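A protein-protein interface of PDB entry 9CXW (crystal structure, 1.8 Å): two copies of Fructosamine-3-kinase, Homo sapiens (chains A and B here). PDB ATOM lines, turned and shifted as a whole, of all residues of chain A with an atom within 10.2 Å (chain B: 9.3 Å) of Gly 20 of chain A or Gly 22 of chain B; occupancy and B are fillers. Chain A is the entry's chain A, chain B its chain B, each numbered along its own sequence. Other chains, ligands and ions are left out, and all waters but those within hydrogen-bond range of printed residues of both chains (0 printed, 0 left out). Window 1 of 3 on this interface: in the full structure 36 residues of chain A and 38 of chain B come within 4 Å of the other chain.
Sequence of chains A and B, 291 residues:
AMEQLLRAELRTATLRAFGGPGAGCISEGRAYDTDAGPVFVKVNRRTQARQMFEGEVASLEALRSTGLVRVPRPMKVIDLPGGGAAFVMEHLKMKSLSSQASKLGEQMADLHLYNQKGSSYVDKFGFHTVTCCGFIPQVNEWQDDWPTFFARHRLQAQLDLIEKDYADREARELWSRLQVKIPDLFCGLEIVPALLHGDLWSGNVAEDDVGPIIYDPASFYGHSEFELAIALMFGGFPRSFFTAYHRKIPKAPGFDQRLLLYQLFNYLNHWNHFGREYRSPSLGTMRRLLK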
ATOM      1  N   MET A   2     -25.586 -28.830  -7.044  1.00  0.00           N
ATOM      2  CA  MET A   2     -24.596 -29.886  -7.214  1.00  0.00           C
ATOM      3  C   MET A   2     -24.943 -31.132  -6.402  1.00  0.00           C
ATOM      4  O   MET A   2     -24.686 -32.251  -6.848  1.00  0.00           O
ATOM      5  CB  MET A   2     -23.205 -29.373  -6.877  1.00  0.00           C
ATOM      6  CG  MET A   2     -22.104 -30.230  -7.499  1.00  0.00           C
ATOM      7  SD  MET A   2     -20.772 -30.287  -6.325  1.00  0.00           S
ATOM      8  CE  MET A   2     -21.703 -30.671  -4.824  1.00  0.00           C
ATOM      9  N   ARG A  16     -24.735 -37.545   2.314  1.00  0.00           N
ATOM     10  CA  ARG A  16     -24.555 -36.871   3.591  1.00  0.00           C
ATOM     11  C   ARG A  16     -23.093 -36.483   3.690  1.00  0.00           C
ATOM     12  O   ARG A  16     -22.222 -37.346   3.836  1.00  0.00           O
ATOM     13  CB  ARG A  16     -24.974 -37.771   4.755  1.00  0.00           C
ATOM     14  N   ALA A  17     -22.842 -35.184   3.625  1.00  0.00           N
ATOM     15  CA  ALA A  17     -21.493 -34.678   3.784  1.00  0.00           C
ATOM     16  C   ALA A  17     -20.937 -35.084   5.143  1.00  0.00           C
ATOM     17  O   ALA A  17     -21.682 -35.313   6.102  1.00  0.00           O
ATOM     18  CB  ALA A  17     -21.487 -33.157   3.643  1.00  0.00           C
ATOM     19  N   PHE A  18     -19.621 -35.260   5.192  1.00  0.00           N
ATOM     20  CA  PHE A  18     -18.911 -35.527   6.438  1.00  0.00           C
ATOM     21  C   PHE A  18     -17.448 -35.165   6.218  1.00  0.00           C
ATOM     22  O   PHE A  18     -17.004 -34.957   5.086  1.00  0.00           O
ATOM     23  CB  PHE A  18     -19.068 -36.977   6.905  1.00  0.00           C
ATOM     24  CG  PHE A  18     -18.296 -37.986   6.071  1.00  0.00           C
ATOM     25  CD1 PHE A  18     -18.870 -38.554   4.942  1.00  0.00           C
ATOM     26  CD2 PHE A  18     -17.009 -38.373   6.423  1.00  0.00           C
ATOM     27  CE1 PHE A  18     -18.182 -39.492   4.181  1.00  0.00           C
ATOM     28  CE2 PHE A  18     -16.317 -39.310   5.663  1.00  0.00           C
ATOM     29  CZ  PHE A  18     -16.909 -39.869   4.549  1.00  0.00           C
ATOM     30  N   GLY A  19     -16.706 -35.068   7.319  1.00  0.00           N
ATOM     31  CA  GLY A  19     -15.302 -34.711   7.248  1.00  0.00           C
ATOM     32  C   GLY A  19     -14.994 -33.258   6.949  1.00  0.00           C
ATOM     33  O   GLY A  19     -13.811 -32.899   6.890  1.00  0.00           O
ATOM     34  N   GLY A  20     -16.009 -32.415   6.753  1.00  0.00           N
ATOM     35  CA  GLY A  20     -15.800 -31.000   6.494  1.00  0.00           C
ATOM     36  C   GLY A  20     -14.952 -30.697   5.272  1.00  0.00           C
ATOM     37  O   GLY A  20     -14.320 -29.640   5.187  1.00  0.00           O
ATOM     38  N   CYS A  25      -3.576 -24.013   3.501  1.00  0.00           N
ATOM     39  CA  CYS A  25      -4.236 -24.028   2.199  1.00  0.00           C
ATOM     40  C   CYS A  25      -4.016 -22.683   1.507  1.00  0.00           C
ATOM     41  O   CYS A  25      -3.316 -21.831   2.049  1.00  0.00           O
ATOM     42  CB  CYS A  25      -5.727 -24.325   2.364  1.00  0.00           C
ATOM     43  SG  CYS A  25      -6.674 -24.369   0.838  1.00  0.00           S
ATOM     44  N   ILE A  26      -4.596 -22.501   0.317  1.00  0.00           N
ATOM     45  CA  ILE A  26      -4.491 -21.253  -0.442  1.00  0.00           C
ATOM     46  C   ILE A  26      -3.030 -20.878  -0.696  1.00  0.00           C
ATOM     47  O   ILE A  26      -2.715 -19.697  -0.889  1.00  0.00           O
ATOM     48  CB  ILE A  26      -5.238 -20.106   0.278  1.00  0.00           C
ATOM     49  N   LEU A  92      -8.589 -22.711  14.233  1.00  0.00           N
ATOM     50  CA  LEU A  92     -10.043 -22.575  14.287  1.00  0.00           C
ATOM     51  C   LEU A  92     -10.640 -23.589  13.320  1.00  0.00           C
ATOM     52  O   LEU A  92     -10.199 -23.681  12.169  1.00  0.00           O
ATOM     53  CB  LEU A  92     -10.483 -21.152  13.893  1.00  0.00           C
ATOM     54  CG  LEU A  92     -10.035 -20.046  14.847  1.00  0.00           C
ATOM     55  CD1 LEU A  92     -10.556 -18.647  14.396  1.00  0.00           C
ATOM     56  CD2 LEU A  92     -10.447 -20.361  16.262  1.00  0.00           C
ATOM     57  N   LYS A  93     -11.608 -24.375  13.798  1.00  0.00           N
ATOM     58  CA  LYS A  93     -12.357 -25.254  12.910  1.00  0.00           C
ATOM     59  C   LYS A  93     -13.311 -24.381  12.114  1.00  0.00           C
ATOM     60  O   LYS A  93     -14.134 -23.674  12.698  1.00  0.00           O
ATOM     61  CB  LYS A  93     -13.113 -26.319  13.711  1.00  0.00           C
ATOM     62  N   MET A  94     -13.223 -24.437  10.786  1.00  0.00           N
ATOM     63  CA  MET A  94     -13.777 -23.375   9.958  1.00  0.00           C
ATOM     64  C   MET A  94     -14.507 -24.020   8.785  1.00  0.00           C
ATOM     65  O   MET A  94     -13.965 -24.927   8.147  1.00  0.00           O
ATOM     66  CB  MET A  94     -12.609 -22.521   9.427  1.00  0.00           C
ATOM     67  CG  MET A  94     -12.177 -21.328  10.285  1.00  0.00           C
ATOM     68  SD  MET A  94     -10.927 -20.381   9.400  1.00  0.00           S
ATOM     69  CE  MET A  94     -11.298 -20.948   7.752  1.00  0.00           C
ATOM     70  N   LYS A  95     -15.704 -23.523   8.475  1.00  0.00           N
ATOM     71  CA  LYS A  95     -16.478 -23.862   7.289  1.00  0.00           C
ATOM     72  C   LYS A  95     -16.797 -22.580   6.523  1.00  0.00           C
ATOM     73  O   LYS A  95     -16.626 -21.473   7.040  1.00  0.00           O
ATOM     74  CB  LYS A  95     -17.776 -24.605   7.669  1.00  0.00           C
ATOM     75  N   SER A  96     -17.240 -22.715   5.271  1.00  0.00           N
ATOM     76  CA  SER A  96     -17.496 -21.522   4.471  1.00  0.00           C
ATOM     77  C   SER A  96     -18.649 -20.706   5.065  1.00  0.00           C
ATOM     78  O   SER A  96     -19.527 -21.222   5.769  1.00  0.00           O
ATOM     79  CB  SER A  96     -17.783 -21.894   3.015  1.00  0.00           C
ATOM     80  OG  SER A  96     -18.463 -23.129   2.952  1.00  0.00           O
ATOM     81  N   GLU A 207     -16.902 -19.571   9.014  1.00  0.00           N
ATOM     82  CA  GLU A 207     -17.682 -19.571  10.241  1.00  0.00           C
ATOM     83  C   GLU A 207     -17.460 -20.889  10.963  1.00  0.00           C
ATOM     84  O   GLU A 207     -16.946 -21.855  10.397  1.00  0.00           O
ATOM     85  CB  GLU A 207     -19.187 -19.337   9.982  1.00  0.00           C
ATOM     86  CG  GLU A 207     -19.862 -20.551   9.337  1.00  0.00           C
ATOM     87  CD  GLU A 207     -21.304 -20.341   8.916  1.00  0.00           C
ATOM     88  OE1 GLU A 207     -21.637 -19.304   8.289  1.00  0.00           O
ATOM     89  OE2 GLU A 207     -22.117 -21.238   9.222  1.00  0.00           O
ATOM     90  N   TYR A 215     -10.078 -13.616   8.589  1.00  0.00           N
ATOM     91  CA  TYR A 215      -8.644 -13.848   8.769  1.00  0.00           C
ATOM     92  C   TYR A 215      -7.877 -13.323   7.566  1.00  0.00           C
ATOM     93  O   TYR A 215      -8.459 -12.789   6.613  1.00  0.00           O
ATOM     94  CB  TYR A 215      -8.373 -15.353   8.977  1.00  0.00           C
ATOM     95  CG  TYR A 215      -9.048 -16.193   7.926  1.00  0.00           C
ATOM     96  CD1 TYR A 215     -10.344 -16.673   8.120  1.00  0.00           C
ATOM     97  CD2 TYR A 215      -8.398 -16.528   6.739  1.00  0.00           C
ATOM     98  CE1 TYR A 215     -10.969 -17.481   7.138  1.00  0.00           C
ATOM     99  CE2 TYR A 215      -9.015 -17.326   5.775  1.00  0.00           C
ATOM    100  CZ  TYR A 215     -10.291 -17.783   5.991  1.00  0.00           C
ATOM    101  OH  TYR A 215     -10.916 -18.533   5.039  1.00  0.00           O
ATOM    102  N   GLY B  19      -5.441 -32.470   8.234  1.00  0.00           N
ATOM    103  CA  GLY B  19      -6.162 -31.742   7.206  1.00  0.00           C
ATOM    104  C   GLY B  19      -5.395 -31.756   5.888  1.00  0.00           C
ATOM    105  O   GLY B  19      -5.961 -31.584   4.805  1.00  0.00           O
ATOM    106  N   GLY B  22     -14.426 -28.401   1.705  1.00  0.00           N
ATOM    107  CA  GLY B  22     -13.330 -27.794   0.970  1.00  0.00           C
ATOM    108  C   GLY B  22     -11.974 -28.298   1.428  1.00  0.00           C
ATOM    109  O   GLY B  22     -11.684 -28.322   2.629  1.00  0.00           O
ATOM    110  N   ALA B  23     -11.142 -28.694   0.462  1.00  0.00           N
ATOM    111  CA  ALA B  23      -9.855 -29.326   0.739  1.00  0.00           C
ATOM    112  C   ALA B  23      -9.001 -29.367  -0.530  1.00  0.00           C
ATOM    113  O   ALA B  23      -9.354 -30.056  -1.496  1.00  0.00           O
ATOM    114  CB  ALA B  23     -10.072 -30.734   1.311  1.00  0.00           C
ATOM    115  N   GLY B  24      -7.890 -28.618  -0.545  1.00  0.00           N
ATOM    116  CA  GLY B  24      -7.027 -28.516  -1.716  1.00  0.00           C
ATOM    117  C   GLY B  24      -6.786 -27.093  -2.203  1.00  0.00           C
ATOM    118  O   GLY B  24      -7.576 -26.200  -1.883  1.00  0.00           O
ATOM    119  N   CYS B  25      -5.707 -26.866  -2.977  1.00  0.00           N
ATOM    120  CA  CYS B  25      -5.385 -25.536  -3.505  1.00  0.00           C
ATOM    121  C   CYS B  25      -5.922 -25.288  -4.910  1.00  0.00           C
ATOM    122  O   CYS B  25      -6.051 -24.125  -5.307  1.00  0.00           O
ATOM    123  CB  CYS B  25      -3.865 -25.299  -3.547  1.00  0.00           C
ATOM    124  SG  CYS B  25      -2.925 -25.774  -2.082  1.00  0.00           S
ATOM    125  N   SER B  27      -8.728 -27.384  -6.352  1.00  0.00           N
ATOM    126  CA  SER B  27     -10.133 -27.743  -6.409  1.00  0.00           C
ATOM    127  C   SER B  27     -10.689 -27.837  -4.997  1.00  0.00           C
ATOM    128  O   SER B  27      -9.949 -27.973  -4.021  1.00  0.00           O
ATOM    129  CB  SER B  27     -10.348 -29.076  -7.146  1.00  0.00           C
ATOM    130  OG  SER B  27      -9.788 -29.021  -8.445  1.00  0.00           O
ATOM    131  N   GLU B  28     -12.012 -27.831  -4.922  1.00  0.00           N
ATOM    132  CA  GLU B  28     -12.734 -27.963  -3.660  1.00  0.00           C
ATOM    133  C   GLU B  28     -13.054 -29.438  -3.462  1.00  0.00           C
ATOM    134  O   GLU B  28     -13.556 -30.079  -4.376  1.00  0.00           O
ATOM    135  CB  GLU B  28     -14.034 -27.164  -3.722  1.00  0.00           C
ATOM    136  CG  GLU B  28     -15.070 -27.596  -2.697  1.00  0.00           C
ATOM    137  CD  GLU B  28     -16.057 -26.507  -2.357  1.00  0.00           C
ATOM    138  OE1 GLU B  28     -16.602 -26.537  -1.227  1.00  0.00           O
ATOM    139  OE2 GLU B  28     -16.288 -25.632  -3.230  1.00  0.00           O
ATOM    140  N   GLY B  29     -12.810 -29.968  -2.269  1.00  0.00           N
ATOM    141  CA  GLY B  29     -13.044 -31.393  -2.110  1.00  0.00           C
ATOM    142  C   GLY B  29     -13.823 -31.729  -0.863  1.00  0.00           C
ATOM    143  O   GLY B  29     -13.579 -31.163   0.205  1.00  0.00           O
ATOM    144  N   ARG B  30     -14.805 -32.618  -1.002  1.00  0.00           N
ATOM    145  CA  ARG B  30     -15.687 -32.944   0.112  1.00  0.00           C
ATOM    146  C   ARG B  30     -16.033 -34.420   0.052  1.00  0.00           C
ATOM    147  O   ARG B  30     -16.181 -34.999  -1.026  1.00  0.00           O
ATOM    148  CB  ARG B  30     -16.977 -32.096   0.095  1.00  0.00           C
ATOM    149  N   ALA B  31     -16.204 -35.010   1.225  1.00  0.00           N
ATOM    150  CA  ALA B  31     -16.586 -36.403   1.356  1.00  0.00           C
ATOM    151  C   ALA B  31     -18.084 -36.508   1.602  1.00  0.00           C
ATOM    152  O   ALA B  31     -18.652 -35.733   2.384  1.00  0.00           O
ATOM    153  CB  ALA B  31     -15.827 -37.046   2.509  1.00  0.00           C
ATOM    154  N   TYR B  32     -18.712 -37.492   0.964  1.00  0.00           N
ATOM    155  CA  TYR B  32     -20.147 -37.712   1.118  1.00  0.00           C
ATOM    156  C   TYR B  32     -20.408 -39.172   1.409  1.00  0.00           C
ATOM    157  O   TYR B  32     -19.749 -40.055   0.855  1.00  0.00           O
ATOM    158  CB  TYR B  32     -20.950 -37.373  -0.109  1.00  0.00           C
ATOM    159  CG  TYR B  32     -20.904 -35.954  -0.511  1.00  0.00           C
ATOM    160  CD1 TYR B  32     -21.839 -35.037  -0.033  1.00  0.00           C
ATOM    161  CD2 TYR B  32     -19.974 -35.535  -1.445  1.00  0.00           C
ATOM    162  CE1 TYR B  32     -21.810 -33.717  -0.435  1.00  0.00           C
ATOM    163  CE2 TYR B  32     -19.933 -34.238  -1.867  1.00  0.00           C
ATOM    164  CZ  TYR B  32     -20.855 -33.326  -1.365  1.00  0.00           C
ATOM    165  OH  TYR B  32     -20.793 -32.040  -1.802  1.00  0.00           O
ATOM    166  N   PHE B  40     -15.431 -39.418  -2.342  1.00  0.00           N
ATOM    167  CA  PHE B  40     -14.777 -38.124  -2.235  1.00  0.00           C
ATOM    168  C   PHE B  40     -14.967 -37.389  -3.551  1.00  0.00           C
ATOM    169  O   PHE B  40     -14.881 -38.002  -4.617  1.00  0.00           O
ATOM    170  CB  PHE B  40     -13.289 -38.285  -1.895  1.00  0.00           C
ATOM    171  CG  PHE B  40     -12.590 -36.980  -1.690  1.00  0.00           C
ATOM    172  CD1 PHE B  40     -12.766 -36.255  -0.513  1.00  0.00           C
ATOM    173  CD2 PHE B  40     -11.778 -36.453  -2.701  1.00  0.00           C
ATOM    174  CE1 PHE B  40     -12.129 -35.009  -0.334  1.00  0.00           C
ATOM    175  CE2 PHE B  40     -11.140 -35.215  -2.543  1.00  0.00           C
ATOM    176  CZ  PHE B  40     -11.314 -34.488  -1.349  1.00  0.00           C
ATOM    177  N   VAL B  41     -15.318 -36.104  -3.498  1.00  0.00           N
ATOM    178  CA  VAL B  41     -15.685 -35.363  -4.707  1.00  0.00           C
ATOM    179  C   VAL B  41     -14.862 -34.090  -4.777  1.00  0.00           C
ATOM    180  O   VAL B  41     -14.914 -33.276  -3.848  1.00  0.00           O
ATOM    181  CB  VAL B  41     -17.181 -34.992  -4.743  1.00  0.00           C
ATOM    182  CG1 VAL B  41     -17.509 -34.312  -6.106  1.00  0.00           C
ATOM    183  CG2 VAL B  41     -18.067 -36.220  -4.478  1.00  0.00           C
ATOM    184  N   LYS B  42     -14.152 -33.905  -5.888  1.00  0.00           N
ATOM    185  CA  LYS B  42     -13.424 -32.682  -6.220  1.00  0.00           C
ATOM    186  C   LYS B  42     -14.229 -31.870  -7.225  1.00  0.00           C
ATOM    187  O   LYS B  42     -14.797 -32.414  -8.168  1.00  0.00           O
ATOM    188  CB  LYS B  42     -12.029 -33.018  -6.788  1.00  0.00           C
ATOM    189  CG  LYS B  42     -11.121 -33.503  -5.666  1.00  0.00           C
ATOM    190  CD  LYS B  42      -9.771 -34.142  -6.094  1.00  0.00           C
ATOM    191  CE  LYS B  42      -8.888 -33.262  -6.924  1.00  0.00           C
ATOM    192  NZ  LYS B  42      -7.586 -34.015  -7.083  1.00  0.00           N
ATOM    193  N   VAL B  43     -14.310 -30.565  -6.986  1.00  0.00           N
ATOM    194  CA  VAL B  43     -15.078 -29.627  -7.797  1.00  0.00           C
ATOM    195  C   VAL B  43     -14.128 -28.562  -8.302  1.00  0.00           C
ATOM    196  O   VAL B  43     -13.346 -27.991  -7.529  1.00  0.00           O
ATOM    197  CB  VAL B  43     -16.227 -28.984  -6.996  1.00  0.00           C
ATOM    198  CG1 VAL B  43     -16.927 -27.924  -7.870  1.00  0.00           C
ATOM    199  CG2 VAL B  43     -17.226 -30.054  -6.587  1.00  0.00           C
ATOM    200  N   HIS B  91     -13.597 -42.937  -1.528  1.00  0.00           N
ATOM    201  CA  HIS B  91     -13.196 -42.244  -0.315  1.00  0.00           C
ATOM    202  C   HIS B  91     -12.207 -43.093   0.462  1.00  0.00           C
ATOM    203  O   HIS B  91     -12.421 -44.297   0.636  1.00  0.00           O
ATOM    204  CB  HIS B  91     -14.404 -41.966   0.593  1.00  0.00           C
ATOM    205  CG  HIS B  91     -14.012 -41.268   1.847  1.00  0.00           C
ATOM    206  ND1 HIS B  91     -13.584 -41.946   2.967  1.00  0.00           N
ATOM    207  CD2 HIS B  91     -13.909 -39.953   2.136  1.00  0.00           C
ATOM    208  CE1 HIS B  91     -13.267 -41.071   3.908  1.00  0.00           C
ATOM    209  NE2 HIS B  91     -13.476 -39.859   3.437  1.00  0.00           N
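Positions printed for both chains: 19 and 25.
Of the 16 printed residues of chain B, 6 touch a printed residue of chain A.
Printed residues of chain B that touch a printed residue of chain A: Gly 22, Gly 24, Ala 31, Tyr 32, Val 43 and His 91.
Hydrophobic or aromatic side chains of chain B that line the printed part of chain A: Ala 31, Tyr 32, Val 43 and His 91.
Of the 15 printed residues of chain A, 6 touch a printed residue of chain B.
Among the printed residues, 10 pairs touch across the chains.
Among the printed residues, no Asp or Glu carboxylate lies within 4 Å of a Lys or Arg side-chain nitrogen of the other chain.
Of chain B, only Gly 22 (3.7 Å) comes within 4 Å of Gly 20 of chain A.
Of chain A, only Gly 20 comes within 4 Å of Gly 22 of chain B.
Ala 23 of chain B touches none of the printed residues of chain A.
No residue of chain A comes within 4 Å of Gly 29 of chain B.
Of the printed residues of chain B, Met 2 of chain A touches Tyr 32 and Val 43.
Of the printed residues of chain B, Arg 16 of chain A touches Tyr 32 (3.4 Å).
Printed residues of chain A within 4 Å of Ala 31 of chain B: Ala 17 and Phe 18.
The nearest printed residue of chain A that does not touch Gly 22 of chain B is Gly 19 of chain A (6.6 Å).
The backbone carbonyl oxygen (O) of Glu 28 of chain B is in hydrogen-bond range of the backbone NH (N) of Val 43 of chain B (2.8 Å).
The backbone carbonyl oxygen (O) of Gly 29 of chain B is in hydrogen-bond range of the backbone NH (N) of Gly 22 of chain B, 3.3 Å away.
SG of Cys 25 of chain A is in hydrogen-bond range of O of Gly 24 of chain B (3.4 Å).
N of Phe 18 of chain A is in hydrogen-bond range of O of Ala 31 of chain B, at 3.0 Å.
CE of Met 2 of chain A touches OH of Tyr 32 of chain B (3.4 Å).
Met 2 of chain A touches Val 43 of chain B (SD to CG2, 3.6 Å).
Arg 16 of chain A touches Tyr 32 of chain B (O to CA, 3.4 Å).
O of Ala 31 of chain B touches CA of Ala 17 of chain A, 3.3 Å away.
Tyr 32 of chain B touches Ala 17 of chain A (CD1 to N, 3.8 Å).
C of Tyr 32 of chain B touches CE1 of Phe 18 of chain A, 3.6 Å away.
Phe 18 of chain A touches His 91 of chain B.
N of Gly 22 of chain B touches O of Gly 20 of chain A, at 3.7 Å.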
